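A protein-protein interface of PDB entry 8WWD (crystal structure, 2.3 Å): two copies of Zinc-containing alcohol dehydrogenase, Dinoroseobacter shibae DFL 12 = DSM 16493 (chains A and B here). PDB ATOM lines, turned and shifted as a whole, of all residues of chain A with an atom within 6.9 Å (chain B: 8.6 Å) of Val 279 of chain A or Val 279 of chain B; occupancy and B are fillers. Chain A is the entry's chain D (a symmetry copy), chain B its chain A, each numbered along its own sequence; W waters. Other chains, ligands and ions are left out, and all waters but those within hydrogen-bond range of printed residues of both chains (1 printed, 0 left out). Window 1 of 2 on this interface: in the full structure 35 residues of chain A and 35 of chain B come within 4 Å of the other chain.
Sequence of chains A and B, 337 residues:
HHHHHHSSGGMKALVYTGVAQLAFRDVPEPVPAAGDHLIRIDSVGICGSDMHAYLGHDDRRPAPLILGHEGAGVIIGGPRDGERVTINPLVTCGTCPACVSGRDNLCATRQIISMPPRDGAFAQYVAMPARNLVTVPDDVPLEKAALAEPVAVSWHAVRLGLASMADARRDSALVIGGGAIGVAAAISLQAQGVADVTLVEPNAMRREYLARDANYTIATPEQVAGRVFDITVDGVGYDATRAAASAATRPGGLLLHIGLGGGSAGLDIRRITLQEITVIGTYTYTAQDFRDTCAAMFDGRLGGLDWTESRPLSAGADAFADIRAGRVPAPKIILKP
The backbone NH (N) of Val 279 of chain B lies within hydrogen-bond range of the backbone carbonyl oxygen (O) of Val 279 of chain A (2.7 Å).
The side-chain hydroxyl (OG1) of Thr 273 of chain B lies within hydrogen-bond range of a ring nitrogen (ND1) of His 257 of chain A, at 3.0 Å.
Leu 267 of chain B touches its own counterpart, Leu 267 of chain A.
Ile 277 of chain A touches Ile 280 of chain B, and with the chains exchanged Ile 280 of chain A touches Ile 277 of chain B.
Thr 278 of chain A touches Val 279 of chain B, and with the chains exchanged Val 279 of chain A touches Thr 278 of chain B.
Thr 278 of chain A touches Ile 280 of chain B, and with the chains exchanged Ile 280 of chain A touches Thr 278 of chain B.
Positions printed for both chains: 246, 253, 254, 255, 256, 257, 267, 272, 277, 278, 279, 280 and 281.
Of the 18 pairs that touch across the chains among the printed residues, 14 have their exchanged pair printed and touching as well.
Water W1 lies within hydrogen-bond range of the side-chain hydroxyl of Thr 278 of chain A and the side-chain hydroxyl of Ser 164 of chain B.
Of the 26 printed residues of chain B, 10 touch a printed residue of chain A.
Along chain B the printed residues that touch a printed residue of chain A span positions 267 to 281.
Printed residues of chain A that touch a printed residue of chain B: His 257, Leu 267, Ile 272, Ile 277, Thr 278, Val 279, Ile 280 and Gly 281.
Hydrophobic or aromatic side chains of chain A that line the printed part of chain B: His 257, Leu 267, Ile 272, Val 279 and Ile 280.
Along chain A the printed residues that touch a printed residue of chain B span positions 257 to 281.
Among the printed residues, 18 pairs touch across the chains.
Among the printed residues, no Asp or Glu carboxylate lies within 4 Å of a Lys or Arg side-chain nitrogen of the other chain.
O of Leu 255 of chain A lies within hydrogen-bond range of N of Ile 280 of chain A (3.0 Å).
The backbone NH (N) of His 257 of chain B is in hydrogen-bond range of the backbone carbonyl oxygen (O) of Ile 280 of chain B, 2.8 Å away.
N of Ile 277 of chain B sits at hydrogen-bond distance from O of Ile 272 of chain B.
The backbone carbonyl oxygen (O) of Glu 276 of chain B sits close to the backbone NH (N) of Gly 252 of chain B (3.2 Å).
N of Thr 278 of chain B sits at hydrogen-bond distance from O of Gly 253 of chain B (3.1 Å).
The backbone NH (N) of His 257 of chain A is in hydrogen-bond range of the backbone carbonyl oxygen (O) of Ile 280 of chain A, at 3.1 Å.
Val 279 of chain A touches three residues of chain B.
Val 279 of chain B touches three residues of chain A.
Printed residues of chain A within 4 Å of Ile 280 of chain B: Ile 277 and Thr 278.
Of the printed residues of chain A, Thr 278 of chain B touches Val 279 and Ile 280.
Printed residues of chain A within 4 Å of Ile 272 of chain B: Gly 281.
Printed residues of chain B within 4 Å of Thr 278 of chain A: Val 279 and Ile 280.
Of the printed residues of chain B, Leu 267 of chain A touches Leu 267.
The nearest printed residue of chain B that does not touch Leu 267 of chain A is Ile 269 of chain B (5.0 Å).
Among the printed residues, merely in contact across the chains: His 257 of chain A with Ile 269 of chain B (3.6 Å), Leu 267 of chain A with Leu 267 of chain B (3.97 Å), Ile 272 of chain A with Gly 281 of chain B (3.5 Å), Ile 277 of chain A with Val 279 of chain B (3.9 Å), Ile 277 of chain A with Ile 280 of chain B (3.8 Å), Ile 277 of chain A with Gly 281 of chain B (3.5 Å), Thr 278 of chain A with Val 279 of chain B (3.7 Å), Thr 278 of chain A with Ile 280 of chain B (3.9 Å), Val 279 of chain A with Ile 277 of chain B (3.9 Å), Val 279 of chain A with Thr 278 of chain B (3.7 Å), Ile 280 of chain A with Ile 277 of chain B (3.9 Å), Ile 280 of chain A with Thr 278 of chain B (3.9 Å), Gly 281 of chain A with Ile 272 of chain B (3.4 Å), Gly 281 of chain A with Thr 273 of chain B (3.9 Å), Gly 281 of chain A with Glu 276 of chain B (3.1 Å) and Gly 281 of chain A with Ile 277 of chain B (3.6 Å).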
ATOM      1  N   SER A 246     -34.875 -18.695  15.388  1.00  0.00           N
ATOM      2  CA  SER A 246     -33.901 -19.470  14.570  1.00  0.00           C
ATOM      3  C   SER A 246     -34.643 -20.345  13.559  1.00  0.00           C
ATOM      4  O   SER A 246     -34.373 -20.227  12.365  1.00  0.00           O
ATOM      5  CB  SER A 246     -33.011 -20.304  15.419  1.00  0.00           C
ATOM      6  OG  SER A 246     -32.282 -19.491  16.310  1.00  0.00           O
ATOM      7  N   GLY A 253     -32.098 -14.964   5.733  1.00  0.00           N
ATOM      8  CA  GLY A 253     -33.087 -14.062   6.344  1.00  0.00           C
ATOM      9  C   GLY A 253     -32.505 -13.274   7.492  1.00  0.00           C
ATOM     10  O   GLY A 253     -31.285 -13.437   7.794  1.00  0.00           O
ATOM     11  N   LEU A 254     -33.340 -12.444   8.113  1.00  0.00           N
ATOM     12  CA  LEU A 254     -32.937 -11.561   9.236  1.00  0.00           C
ATOM     13  C   LEU A 254     -33.579 -12.069  10.527  1.00  0.00           C
ATOM     14  O   LEU A 254     -34.755 -12.420  10.488  1.00  0.00           O
ATOM     15  CB  LEU A 254     -33.370 -10.134   8.906  1.00  0.00           C
ATOM     16  CG  LEU A 254     -33.310  -9.130  10.061  1.00  0.00           C
ATOM     17  CD1 LEU A 254     -31.874  -8.895  10.502  1.00  0.00           C
ATOM     18  CD2 LEU A 254     -33.959  -7.826   9.633  1.00  0.00           C
ATOM     19  N   LEU A 255     -32.799 -12.139  11.598  1.00  0.00           N
ATOM     20  CA  LEU A 255     -33.263 -12.413  12.978  1.00  0.00           C
ATOM     21  C   LEU A 255     -32.868 -11.212  13.837  1.00  0.00           C
ATOM     22  O   LEU A 255     -31.655 -11.085  14.146  1.00  0.00           O
ATOM     23  CB  LEU A 255     -32.616 -13.694  13.495  1.00  0.00           C
ATOM     24  CG  LEU A 255     -33.201 -14.296  14.775  1.00  0.00           C
ATOM     25  CD1 LEU A 255     -32.767 -15.738  14.922  1.00  0.00           C
ATOM     26  CD2 LEU A 255     -32.806 -13.504  16.021  1.00  0.00           C
ATOM     27  N   LEU A 256     -33.838 -10.351  14.167  1.00  0.00           N
ATOM     28  CA  LEU A 256     -33.605  -9.204  15.076  1.00  0.00           C
ATOM     29  C   LEU A 256     -33.880  -9.647  16.513  1.00  0.00           C
ATOM     30  O   LEU A 256     -34.954 -10.212  16.781  1.00  0.00           O
ATOM     31  CB  LEU A 256     -34.487  -8.029  14.668  1.00  0.00           C
ATOM     32  CG  LEU A 256     -34.030  -7.279  13.422  1.00  0.00           C
ATOM     33  CD1 LEU A 256     -35.171  -6.439  12.875  1.00  0.00           C
ATOM     34  CD2 LEU A 256     -32.799  -6.423  13.701  1.00  0.00           C
ATOM     35  N   HIS A 257     -32.906  -9.447  17.389  1.00  0.00           N
ATOM     36  CA  HIS A 257     -32.966  -9.833  18.820  1.00  0.00           C
ATOM     37  C   HIS A 257     -32.983  -8.571  19.688  1.00  0.00           C
ATOM     38  O   HIS A 257     -31.893  -8.026  19.917  1.00  0.00           O
ATOM     39  CB  HIS A 257     -31.788 -10.740  19.187  1.00  0.00           C
ATOM     40  CG  HIS A 257     -31.930 -11.307  20.554  1.00  0.00           C
ATOM     41  ND1 HIS A 257     -31.286 -10.776  21.662  1.00  0.00           N
ATOM     42  CD2 HIS A 257     -32.698 -12.313  21.019  1.00  0.00           C
ATOM     43  CE1 HIS A 257     -31.609 -11.476  22.730  1.00  0.00           C
ATOM     44  NE2 HIS A 257     -32.480 -12.406  22.370  1.00  0.00           N
ATOM     45  N   LEU A 267     -30.090 -19.812  20.279  1.00  0.00           N
ATOM     46  CA  LEU A 267     -29.736 -19.730  18.843  1.00  0.00           C
ATOM     47  C   LEU A 267     -29.298 -21.106  18.346  1.00  0.00           C
ATOM     48  O   LEU A 267     -28.433 -21.715  18.997  1.00  0.00           O
ATOM     49  CB  LEU A 267     -28.623 -18.703  18.638  1.00  0.00           C
ATOM     50  CG  LEU A 267     -29.065 -17.245  18.704  1.00  0.00           C
ATOM     51  CD1 LEU A 267     -27.867 -16.331  18.502  1.00  0.00           C
ATOM     52  CD2 LEU A 267     -30.135 -16.948  17.663  1.00  0.00           C
ATOM     53  N   ILE A 272     -28.021 -21.255  11.542  1.00  0.00           N
ATOM     54  CA  ILE A 272     -27.601 -19.865  11.214  1.00  0.00           C
ATOM     55  C   ILE A 272     -26.381 -19.929  10.303  1.00  0.00           C
ATOM     56  O   ILE A 272     -26.243 -19.025   9.484  1.00  0.00           O
ATOM     57  CB  ILE A 272     -27.353 -19.055  12.499  1.00  0.00           C
ATOM     58  CG1 ILE A 272     -28.689 -18.851  13.212  1.00  0.00           C
ATOM     59  CG2 ILE A 272     -26.648 -17.742  12.187  1.00  0.00           C
ATOM     60  CD1 ILE A 272     -28.586 -18.201  14.547  1.00  0.00           C
ATOM     61  N   ILE A 277     -27.940 -17.024   8.129  1.00  0.00           N
ATOM     62  CA  ILE A 277     -28.914 -16.076   8.733  1.00  0.00           C
ATOM     63  C   ILE A 277     -28.138 -14.877   9.295  1.00  0.00           C
ATOM     64  O   ILE A 277     -27.051 -15.068   9.900  1.00  0.00           O
ATOM     65  CB  ILE A 277     -29.777 -16.807   9.775  1.00  0.00           C
ATOM     66  CG1 ILE A 277     -30.817 -17.696   9.087  1.00  0.00           C
ATOM     67  CG2 ILE A 277     -30.430 -15.829  10.729  1.00  0.00           C
ATOM     68  CD1 ILE A 277     -31.399 -18.793   9.954  1.00  0.00           C
ATOM     69  N   THR A 278     -28.628 -13.671   9.018  1.00  0.00           N
ATOM     70  CA  THR A 278     -28.089 -12.422   9.609  1.00  0.00           C
ATOM     71  C   THR A 278     -28.795 -12.231  10.951  1.00  0.00           C
ATOM     72  O   THR A 278     -30.021 -12.025  10.954  1.00  0.00           O
ATOM     73  CB  THR A 278     -28.204 -11.230   8.648  1.00  0.00           C
ATOM     74  OG1 THR A 278     -27.452 -11.479   7.462  1.00  0.00           O
ATOM     75  CG2 THR A 278     -27.692  -9.946   9.260  1.00  0.00           C
ATOM     76  N   VAL A 279     -28.054 -12.409  12.050  1.00  0.00           N
ATOM     77  CA  VAL A 279     -28.541 -12.170  13.437  1.00  0.00           C
ATOM     78  C   VAL A 279     -28.008 -10.823  13.937  1.00  0.00           C
ATOM     79  O   VAL A 279     -26.794 -10.650  14.011  1.00  0.00           O
ATOM     80  CB  VAL A 279     -28.121 -13.318  14.358  1.00  0.00           C
ATOM     81  CG1 VAL A 279     -28.498 -13.058  15.810  1.00  0.00           C
ATOM     82  CG2 VAL A 279     -28.689 -14.642  13.869  1.00  0.00           C
ATOM     83  N   ILE A 280     -28.894  -9.907  14.320  1.00  0.00           N
ATOM     84  CA  ILE A 280     -28.497  -8.557  14.809  1.00  0.00           C
ATOM     85  C   ILE A 280     -29.192  -8.291  16.137  1.00  0.00           C
ATOM     86  O   ILE A 280     -30.420  -8.102  16.123  1.00  0.00           O
ATOM     87  CB  ILE A 280     -28.834  -7.480  13.768  1.00  0.00           C
ATOM     88  CG1 ILE A 280     -28.073  -7.727  12.462  1.00  0.00           C
ATOM     89  CG2 ILE A 280     -28.565  -6.096  14.344  1.00  0.00           C
ATOM     90  CD1 ILE A 280     -28.461  -6.838  11.324  1.00  0.00           C
ATOM     91  N   GLY A 281     -28.426  -8.280  17.229  1.00  0.00           N
ATOM     92  CA  GLY A 281     -28.866  -7.713  18.517  1.00  0.00           C
ATOM     93  C   GLY A 281     -28.959  -6.202  18.397  1.00  0.00           C
ATOM     94  O   GLY A 281     -28.102  -5.634  17.698  1.00  0.00           O
ATOM     95  N   GLY B 161     -20.154 -10.015   4.916  1.00  0.00           N
ATOM     96  CA  GLY B 161     -19.978  -9.294   6.183  1.00  0.00           C
ATOM     97  C   GLY B 161     -19.719  -7.816   5.952  1.00  0.00           C
ATOM     98  O   GLY B 161     -20.458  -6.987   6.525  1.00  0.00           O
ATOM     99  N   SER B 164     -22.691  -5.949   4.782  1.00  0.00           N
ATOM    100  CA  SER B 164     -23.799  -6.020   5.772  1.00  0.00           C
ATOM    101  C   SER B 164     -23.529  -5.120   6.990  1.00  0.00           C
ATOM    102  O   SER B 164     -24.468  -4.895   7.778  1.00  0.00           O
ATOM    103  CB  SER B 164     -24.045  -7.462   6.216  1.00  0.00           C
ATOM    104  OG  SER B 164     -24.505  -8.270   5.130  1.00  0.00           O
ATOM    105  N   THR B 232     -14.567  -9.690  13.645  1.00  0.00           N
ATOM    106  CA  THR B 232     -14.069 -10.984  14.119  1.00  0.00           C
ATOM    107  C   THR B 232     -14.576 -12.059  13.159  1.00  0.00           C
ATOM    108  O   THR B 232     -15.660 -11.923  12.613  1.00  0.00           O
ATOM    109  CB  THR B 232     -14.504 -11.281  15.559  1.00  0.00           C
ATOM    110  OG1 THR B 232     -15.929 -11.340  15.550  1.00  0.00           O
ATOM    111  CG2 THR B 232     -14.004 -10.258  16.561  1.00  0.00           C
ATOM    112  N   ARG B 242     -16.597 -18.942  19.784  1.00  0.00           N
ATOM    113  CA  ARG B 242     -17.775 -18.036  19.657  1.00  0.00           C
ATOM    114  C   ARG B 242     -17.747 -17.004  20.781  1.00  0.00           C
ATOM    115  O   ARG B 242     -17.997 -15.821  20.510  1.00  0.00           O
ATOM    116  CB  ARG B 242     -19.108 -18.782  19.704  1.00  0.00           C
ATOM    117  CG  ARG B 242     -19.597 -19.265  18.347  1.00  0.00           C
ATOM    118  CD  ARG B 242     -20.719 -20.280  18.543  1.00  0.00           C
ATOM    119  NE  ARG B 242     -20.433 -21.335  17.614  1.00  0.00           N
ATOM    120  CZ  ARG B 242     -20.188 -22.596  17.892  1.00  0.00           C
ATOM    121  NH1 ARG B 242     -20.288 -23.074  19.119  1.00  0.00           N
ATOM    122  NH2 ARG B 242     -19.915 -23.401  16.886  1.00  0.00           N
ATOM    123  N   ALA B 245     -14.807 -14.577  20.097  1.00  0.00           N
ATOM    124  CA  ALA B 245     -15.244 -13.637  19.031  1.00  0.00           C
ATOM    125  C   ALA B 245     -16.281 -12.627  19.568  1.00  0.00           C
ATOM    126  O   ALA B 245     -16.209 -11.433  19.186  1.00  0.00           O
ATOM    127  CB  ALA B 245     -15.765 -14.393  17.830  1.00  0.00           C
ATOM    128  N   SER B 246     -17.255 -13.057  20.372  1.00  0.00           N
ATOM    129  CA  SER B 246     -18.215 -12.135  21.050  1.00  0.00           C
ATOM    130  C   SER B 246     -17.442 -11.040  21.799  1.00  0.00           C
ATOM    131  O   SER B 246     -17.618  -9.861  21.483  1.00  0.00           O
ATOM    132  CB  SER B 246     -19.169 -12.854  21.989  1.00  0.00           C
ATOM    133  OG  SER B 246     -19.926 -13.841  21.303  1.00  0.00           O
ATOM    134  N   THR B 249     -15.367  -8.438  19.595  1.00  0.00           N
ATOM    135  CA  THR B 249     -16.084  -7.610  18.596  1.00  0.00           C
ATOM    136  C   THR B 249     -16.460  -6.287  19.264  1.00  0.00           C
ATOM    137  O   THR B 249     -16.988  -6.338  20.376  1.00  0.00           O
ATOM    138  CB  THR B 249     -17.287  -8.350  17.998  1.00  0.00           C
ATOM    139  OG1 THR B 249     -16.857  -9.644  17.553  1.00  0.00           O
ATOM    140  CG2 THR B 249     -17.933  -7.578  16.866  1.00  0.00           C
ATOM    141  N   GLY B 252     -21.376  -2.501  17.678  1.00  0.00           N
ATOM    142  CA  GLY B 252     -21.828  -2.246  16.297  1.00  0.00           C
ATOM    143  C   GLY B 252     -20.977  -2.969  15.264  1.00  0.00           C
ATOM    144  O   GLY B 252     -21.237  -2.770  14.070  1.00  0.00           O
ATOM    145  N   GLY B 253     -19.981  -3.752  15.681  1.00  0.00           N
ATOM    146  CA  GLY B 253     -19.063  -4.417  14.733  1.00  0.00           C
ATOM    147  C   GLY B 253     -19.672  -5.680  14.124  1.00  0.00           C
ATOM    148  O   GLY B 253     -20.908  -5.922  14.255  1.00  0.00           O
ATOM    149  N   LEU B 254     -18.823  -6.502  13.515  1.00  0.00           N
ATOM    150  CA  LEU B 254     -19.253  -7.689  12.736  1.00  0.00           C
ATOM    151  C   LEU B 254     -18.540  -8.907  13.283  1.00  0.00           C
ATOM    152  O   LEU B 254     -17.322  -8.852  13.418  1.00  0.00           O
ATOM    153  CB  LEU B 254     -18.929  -7.508  11.251  1.00  0.00           C
ATOM    154  CG  LEU B 254     -19.064  -8.783  10.415  1.00  0.00           C
ATOM    155  CD1 LEU B 254     -20.520  -9.124  10.204  1.00  0.00           C
ATOM    156  CD2 LEU B 254     -18.366  -8.625   9.081  1.00  0.00           C
ATOM    157  N   LEU B 255     -19.314  -9.949  13.572  1.00  0.00           N
ATOM    158  CA  LEU B 255     -18.830 -11.290  13.965  1.00  0.00           C
ATOM    159  C   LEU B 255     -19.285 -12.263  12.865  1.00  0.00           C
ATOM    160  O   LEU B 255     -20.502 -12.530  12.744  1.00  0.00           O
ATOM    161  CB  LEU B 255     -19.425 -11.632  15.335  1.00  0.00           C
ATOM    162  CG  LEU B 255     -18.840 -12.839  16.065  1.00  0.00           C
ATOM    163  CD1 LEU B 255     -19.336 -12.851  17.495  1.00  0.00           C
ATOM    164  CD2 LEU B 255     -19.179 -14.170  15.385  1.00  0.00           C
ATOM    165  N   LEU B 256     -18.351 -12.705  12.035  1.00  0.00           N
ATOM    166  CA  LEU B 256     -18.618 -13.715  10.983  1.00  0.00           C
ATOM    167  C   LEU B 256     -18.348 -15.081  11.601  1.00  0.00           C
ATOM    168  O   LEU B 256     -17.292 -15.243  12.246  1.00  0.00           O
ATOM    169  CB  LEU B 256     -17.715 -13.466   9.777  1.00  0.00           C
ATOM    170  CG  LEU B 256     -18.114 -12.329   8.853  1.00  0.00           C
ATOM    171  CD1 LEU B 256     -16.981 -12.017   7.893  1.00  0.00           C
ATOM    172  CD2 LEU B 256     -19.386 -12.655   8.076  1.00  0.00           C
ATOM    173  N   HIS B 257     -19.286 -16.006  11.481  1.00  0.00           N
ATOM    174  CA  HIS B 257     -19.151 -17.376  12.032  1.00  0.00           C
ATOM    175  C   HIS B 257     -19.084 -18.387  10.882  1.00  0.00           C
ATOM    176  O   HIS B 257     -20.119 -18.659  10.282  1.00  0.00           O
ATOM    177  CB  HIS B 257     -20.301 -17.683  12.986  1.00  0.00           C
ATOM    178  CG  HIS B 257     -20.152 -19.026  13.614  1.00  0.00           C
ATOM    179  ND1 HIS B 257     -20.729 -20.153  13.078  1.00  0.00           N
ATOM    180  CD2 HIS B 257     -19.475 -19.419  14.715  1.00  0.00           C
ATOM    181  CE1 HIS B 257     -20.434 -21.186  13.842  1.00  0.00           C
ATOM    182  NE2 HIS B 257     -19.647 -20.768  14.844  1.00  0.00           N
ATOM    183  N   LEU B 267     -21.805 -17.894  22.101  1.00  0.00           N
ATOM    184  CA  LEU B 267     -22.118 -16.486  21.757  1.00  0.00           C
ATOM    185  C   LEU B 267     -22.641 -15.810  23.026  1.00  0.00           C
ATOM    186  O   LEU B 267     -23.543 -16.349  23.643  1.00  0.00           O
ATOM    187  CB  LEU B 267     -23.180 -16.410  20.655  1.00  0.00           C
ATOM    188  CG  LEU B 267     -22.728 -16.750  19.238  1.00  0.00           C
ATOM    189  CD1 LEU B 267     -23.940 -16.921  18.336  1.00  0.00           C
ATOM    190  CD2 LEU B 267     -21.811 -15.672  18.683  1.00  0.00           C
ATOM    191  N   ASP B 268     -22.037 -14.692  23.407  1.00  0.00           N
ATOM    192  CA  ASP B 268     -22.498 -13.827  24.513  1.00  0.00           C
ATOM    193  C   ASP B 268     -23.687 -13.042  23.990  1.00  0.00           C
ATOM    194  O   ASP B 268     -23.486 -11.940  23.444  1.00  0.00           O
ATOM    195  CB  ASP B 268     -21.408 -12.879  24.990  1.00  0.00           C
ATOM    196  CG  ASP B 268     -21.855 -12.057  26.183  1.00  0.00           C
ATOM    197  OD1 ASP B 268     -23.069 -11.750  26.264  1.00  0.00           O
ATOM    198  OD2 ASP B 268     -20.975 -11.701  26.991  1.00  0.00           O
ATOM    199  N   ILE B 269     -24.875 -13.617  24.131  1.00  0.00           N
ATOM    200  CA  ILE B 269     -26.133 -13.037  23.578  1.00  0.00           C
ATOM    201  C   ILE B 269     -26.412 -11.680  24.205  1.00  0.00           C
ATOM    202  O   ILE B 269     -27.029 -10.850  23.536  1.00  0.00           O
ATOM    203  CB  ILE B 269     -27.340 -13.953  23.805  1.00  0.00           C
ATOM    204  CG1 ILE B 269     -27.000 -15.383  23.383  1.00  0.00           C
ATOM    205  CG2 ILE B 269     -28.567 -13.393  23.093  1.00  0.00           C
ATOM    206  CD1 ILE B 269     -28.146 -16.333  23.497  1.00  0.00           C
ATOM    207  N   ARG B 271     -24.354  -9.332  25.290  1.00  0.00           N
ATOM    208  CA  ARG B 271     -23.407  -8.345  24.709  1.00  0.00           C
ATOM    209  C   ARG B 271     -23.784  -8.092  23.242  1.00  0.00           C
ATOM    210  O   ARG B 271     -23.835  -6.912  22.826  1.00  0.00           O
ATOM    211  CB  ARG B 271     -21.972  -8.842  24.881  1.00  0.00           C
ATOM    212  CG  ARG B 271     -20.968  -8.018  24.095  1.00  0.00           C
ATOM    213  CD  ARG B 271     -19.538  -8.514  24.206  1.00  0.00           C
ATOM    214  NE  ARG B 271     -18.745  -7.574  23.433  1.00  0.00           N
ATOM    215  CZ  ARG B 271     -18.247  -6.427  23.904  1.00  0.00           C
ATOM    216  NH1 ARG B 271     -18.375  -6.127  25.186  1.00  0.00           N
ATOM    217  NH2 ARG B 271     -17.602  -5.594  23.096  1.00  0.00           N
ATOM    218  N   ILE B 272     -24.092  -9.140  22.475  1.00  0.00           N
ATOM    219  CA  ILE B 272     -24.549  -8.952  21.068  1.00  0.00           C
ATOM    220  C   ILE B 272     -25.729  -7.982  21.090  1.00  0.00           C
ATOM    221  O   ILE B 272     -25.881  -7.193  20.141  1.00  0.00           O
ATOM    222  CB  ILE B 272     -24.887 -10.300  20.394  1.00  0.00           C
ATOM    223  CG1 ILE B 272     -23.616 -11.048  19.988  1.00  0.00           C
ATOM    224  CG2 ILE B 272     -25.803 -10.130  19.200  1.00  0.00           C
ATOM    225  CD1 ILE B 272     -23.759 -12.538  20.076  1.00  0.00           C
ATOM    226  N   THR B 273     -26.541  -8.037  22.142  1.00  0.00           N
ATOM    227  CA  THR B 273     -27.762  -7.211  22.265  1.00  0.00           C
ATOM    228  C   THR B 273     -27.363  -5.786  22.668  1.00  0.00           C
ATOM    229  O   THR B 273     -27.622  -4.841  21.883  1.00  0.00           O
ATOM    230  CB  THR B 273     -28.743  -7.850  23.254  1.00  0.00           C
ATOM    231  OG1 THR B 273     -28.986  -9.190  22.805  1.00  0.00           O
ATOM    232  CG2 THR B 273     -30.012  -7.029  23.385  1.00  0.00           C
ATOM    233  N   GLU B 276     -25.002  -4.216  20.216  1.00  0.00           N
ATOM    234  CA  GLU B 276     -25.540  -4.217  18.833  1.00  0.00           C
ATOM    235  C   GLU B 276     -24.495  -4.828  17.886  1.00  0.00           C
ATOM    236  O   GLU B 276     -24.059  -4.146  16.937  1.00  0.00           O
ATOM    237  CB  GLU B 276     -25.921  -2.786  18.453  1.00  0.00           C
ATOM    238  CG  GLU B 276     -26.847  -2.679  17.269  1.00  0.00           C
ATOM    239  CD  GLU B 276     -27.543  -1.334  17.175  1.00  0.00           C
ATOM    240  OE1 GLU B 276     -27.241  -0.571  16.229  1.00  0.00           O
ATOM    241  OE2 GLU B 276     -28.394  -1.052  18.052  1.00  0.00           O
ATOM    242  N   ILE B 277     -24.085  -6.067  18.138  1.00  0.00           N
ATOM    243  CA  ILE B 277     -23.176  -6.795  17.212  1.00  0.00           C
ATOM    244  C   ILE B 277     -23.997  -7.456  16.090  1.00  0.00           C
ATOM    245  O   ILE B 277     -24.979  -8.140  16.389  1.00  0.00           O
ATOM    246  CB  ILE B 277     -22.328  -7.792  18.005  1.00  0.00           C
ATOM    247  CG1 ILE B 277     -21.375  -7.041  18.934  1.00  0.00           C
ATOM    248  CG2 ILE B 277     -21.588  -8.735  17.075  1.00  0.00           C
ATOM    249  CD1 ILE B 277     -20.743  -7.899  19.999  1.00  0.00           C
ATOM    250  N   THR B 278     -23.617  -7.219  14.830  1.00  0.00           N
ATOM    251  CA  THR B 278     -24.107  -7.985  13.658  1.00  0.00           C
ATOM    252  C   THR B 278     -23.390  -9.340  13.603  1.00  0.00           C
ATOM    253  O   THR B 278     -22.161  -9.359  13.424  1.00  0.00           O
ATOM    254  CB  THR B 278     -23.897  -7.217  12.357  1.00  0.00           C
ATOM    255  OG1 THR B 278     -24.570  -5.963  12.423  1.00  0.00           O
ATOM    256  CG2 THR B 278     -24.422  -7.993  11.167  1.00  0.00           C
ATOM    257  N   VAL B 279     -24.128 -10.430  13.810  1.00  0.00           N
ATOM    258  CA  VAL B 279     -23.598 -11.820  13.788  1.00  0.00           C
ATOM    259  C   VAL B 279     -24.106 -12.500  12.522  1.00  0.00           C
ATOM    260  O   VAL B 279     -25.357 -12.591  12.393  1.00  0.00           O
ATOM    261  CB  VAL B 279     -24.037 -12.607  15.029  1.00  0.00           C
ATOM    262  CG1 VAL B 279     -23.537 -14.045  14.963  1.00  0.00           C
ATOM    263  CG2 VAL B 279     -23.582 -11.925  16.318  1.00  0.00           C
ATOM    264  N   ILE B 280     -23.204 -12.951  11.633  1.00  0.00           N
ATOM    265  CA  ILE B 280     -23.609 -13.630  10.365  1.00  0.00           C
ATOM    266  C   ILE B 280     -22.907 -14.985  10.274  1.00  0.00           C
ATOM    267  O   ILE B 280     -21.643 -15.029  10.224  1.00  0.00           O
ATOM    268  CB  ILE B 280     -23.314 -12.750   9.139  1.00  0.00           C
ATOM    269  CG1 ILE B 280     -24.019 -11.395   9.211  1.00  0.00           C
ATOM    270  CG2 ILE B 280     -23.675 -13.478   7.855  1.00  0.00           C
ATOM    271  CD1 ILE B 280     -23.520 -10.419   8.194  1.00  0.00           C
ATOM    272  N   GLY B 281     -23.691 -16.060  10.304  1.00  0.00           N
ATOM    273  CA  GLY B 281     -23.227 -17.386   9.865  1.00  0.00           C
ATOM    274  C   GLY B 281     -23.180 -17.432   8.342  1.00  0.00           C
ATOM    275  O   GLY B 281     -24.050 -16.800   7.716  1.00  0.00           O
ATOM    276  N   THR B 282     -22.203 -18.118   7.749  1.00  0.00           N
ATOM    277  CA  THR B 282     -22.012 -18.107   6.276  1.00  0.00           C
ATOM    278  C   THR B 282     -21.906 -19.531   5.762  1.00  0.00           C
ATOM    279  O   THR B 282     -21.318 -20.351   6.447  1.00  0.00           O
ATOM    280  CB  THR B 282     -20.810 -17.259   5.839  1.00  0.00           C
ATOM    281  OG1 THR B 282     -19.585 -17.911   6.167  1.00  0.00           O
ATOM    282  CG2 THR B 282     -20.820 -15.897   6.492  1.00  0.00           C
HETATM  283  O   HOH W   1     -26.727  -9.570   5.893  1.00  0.00           O
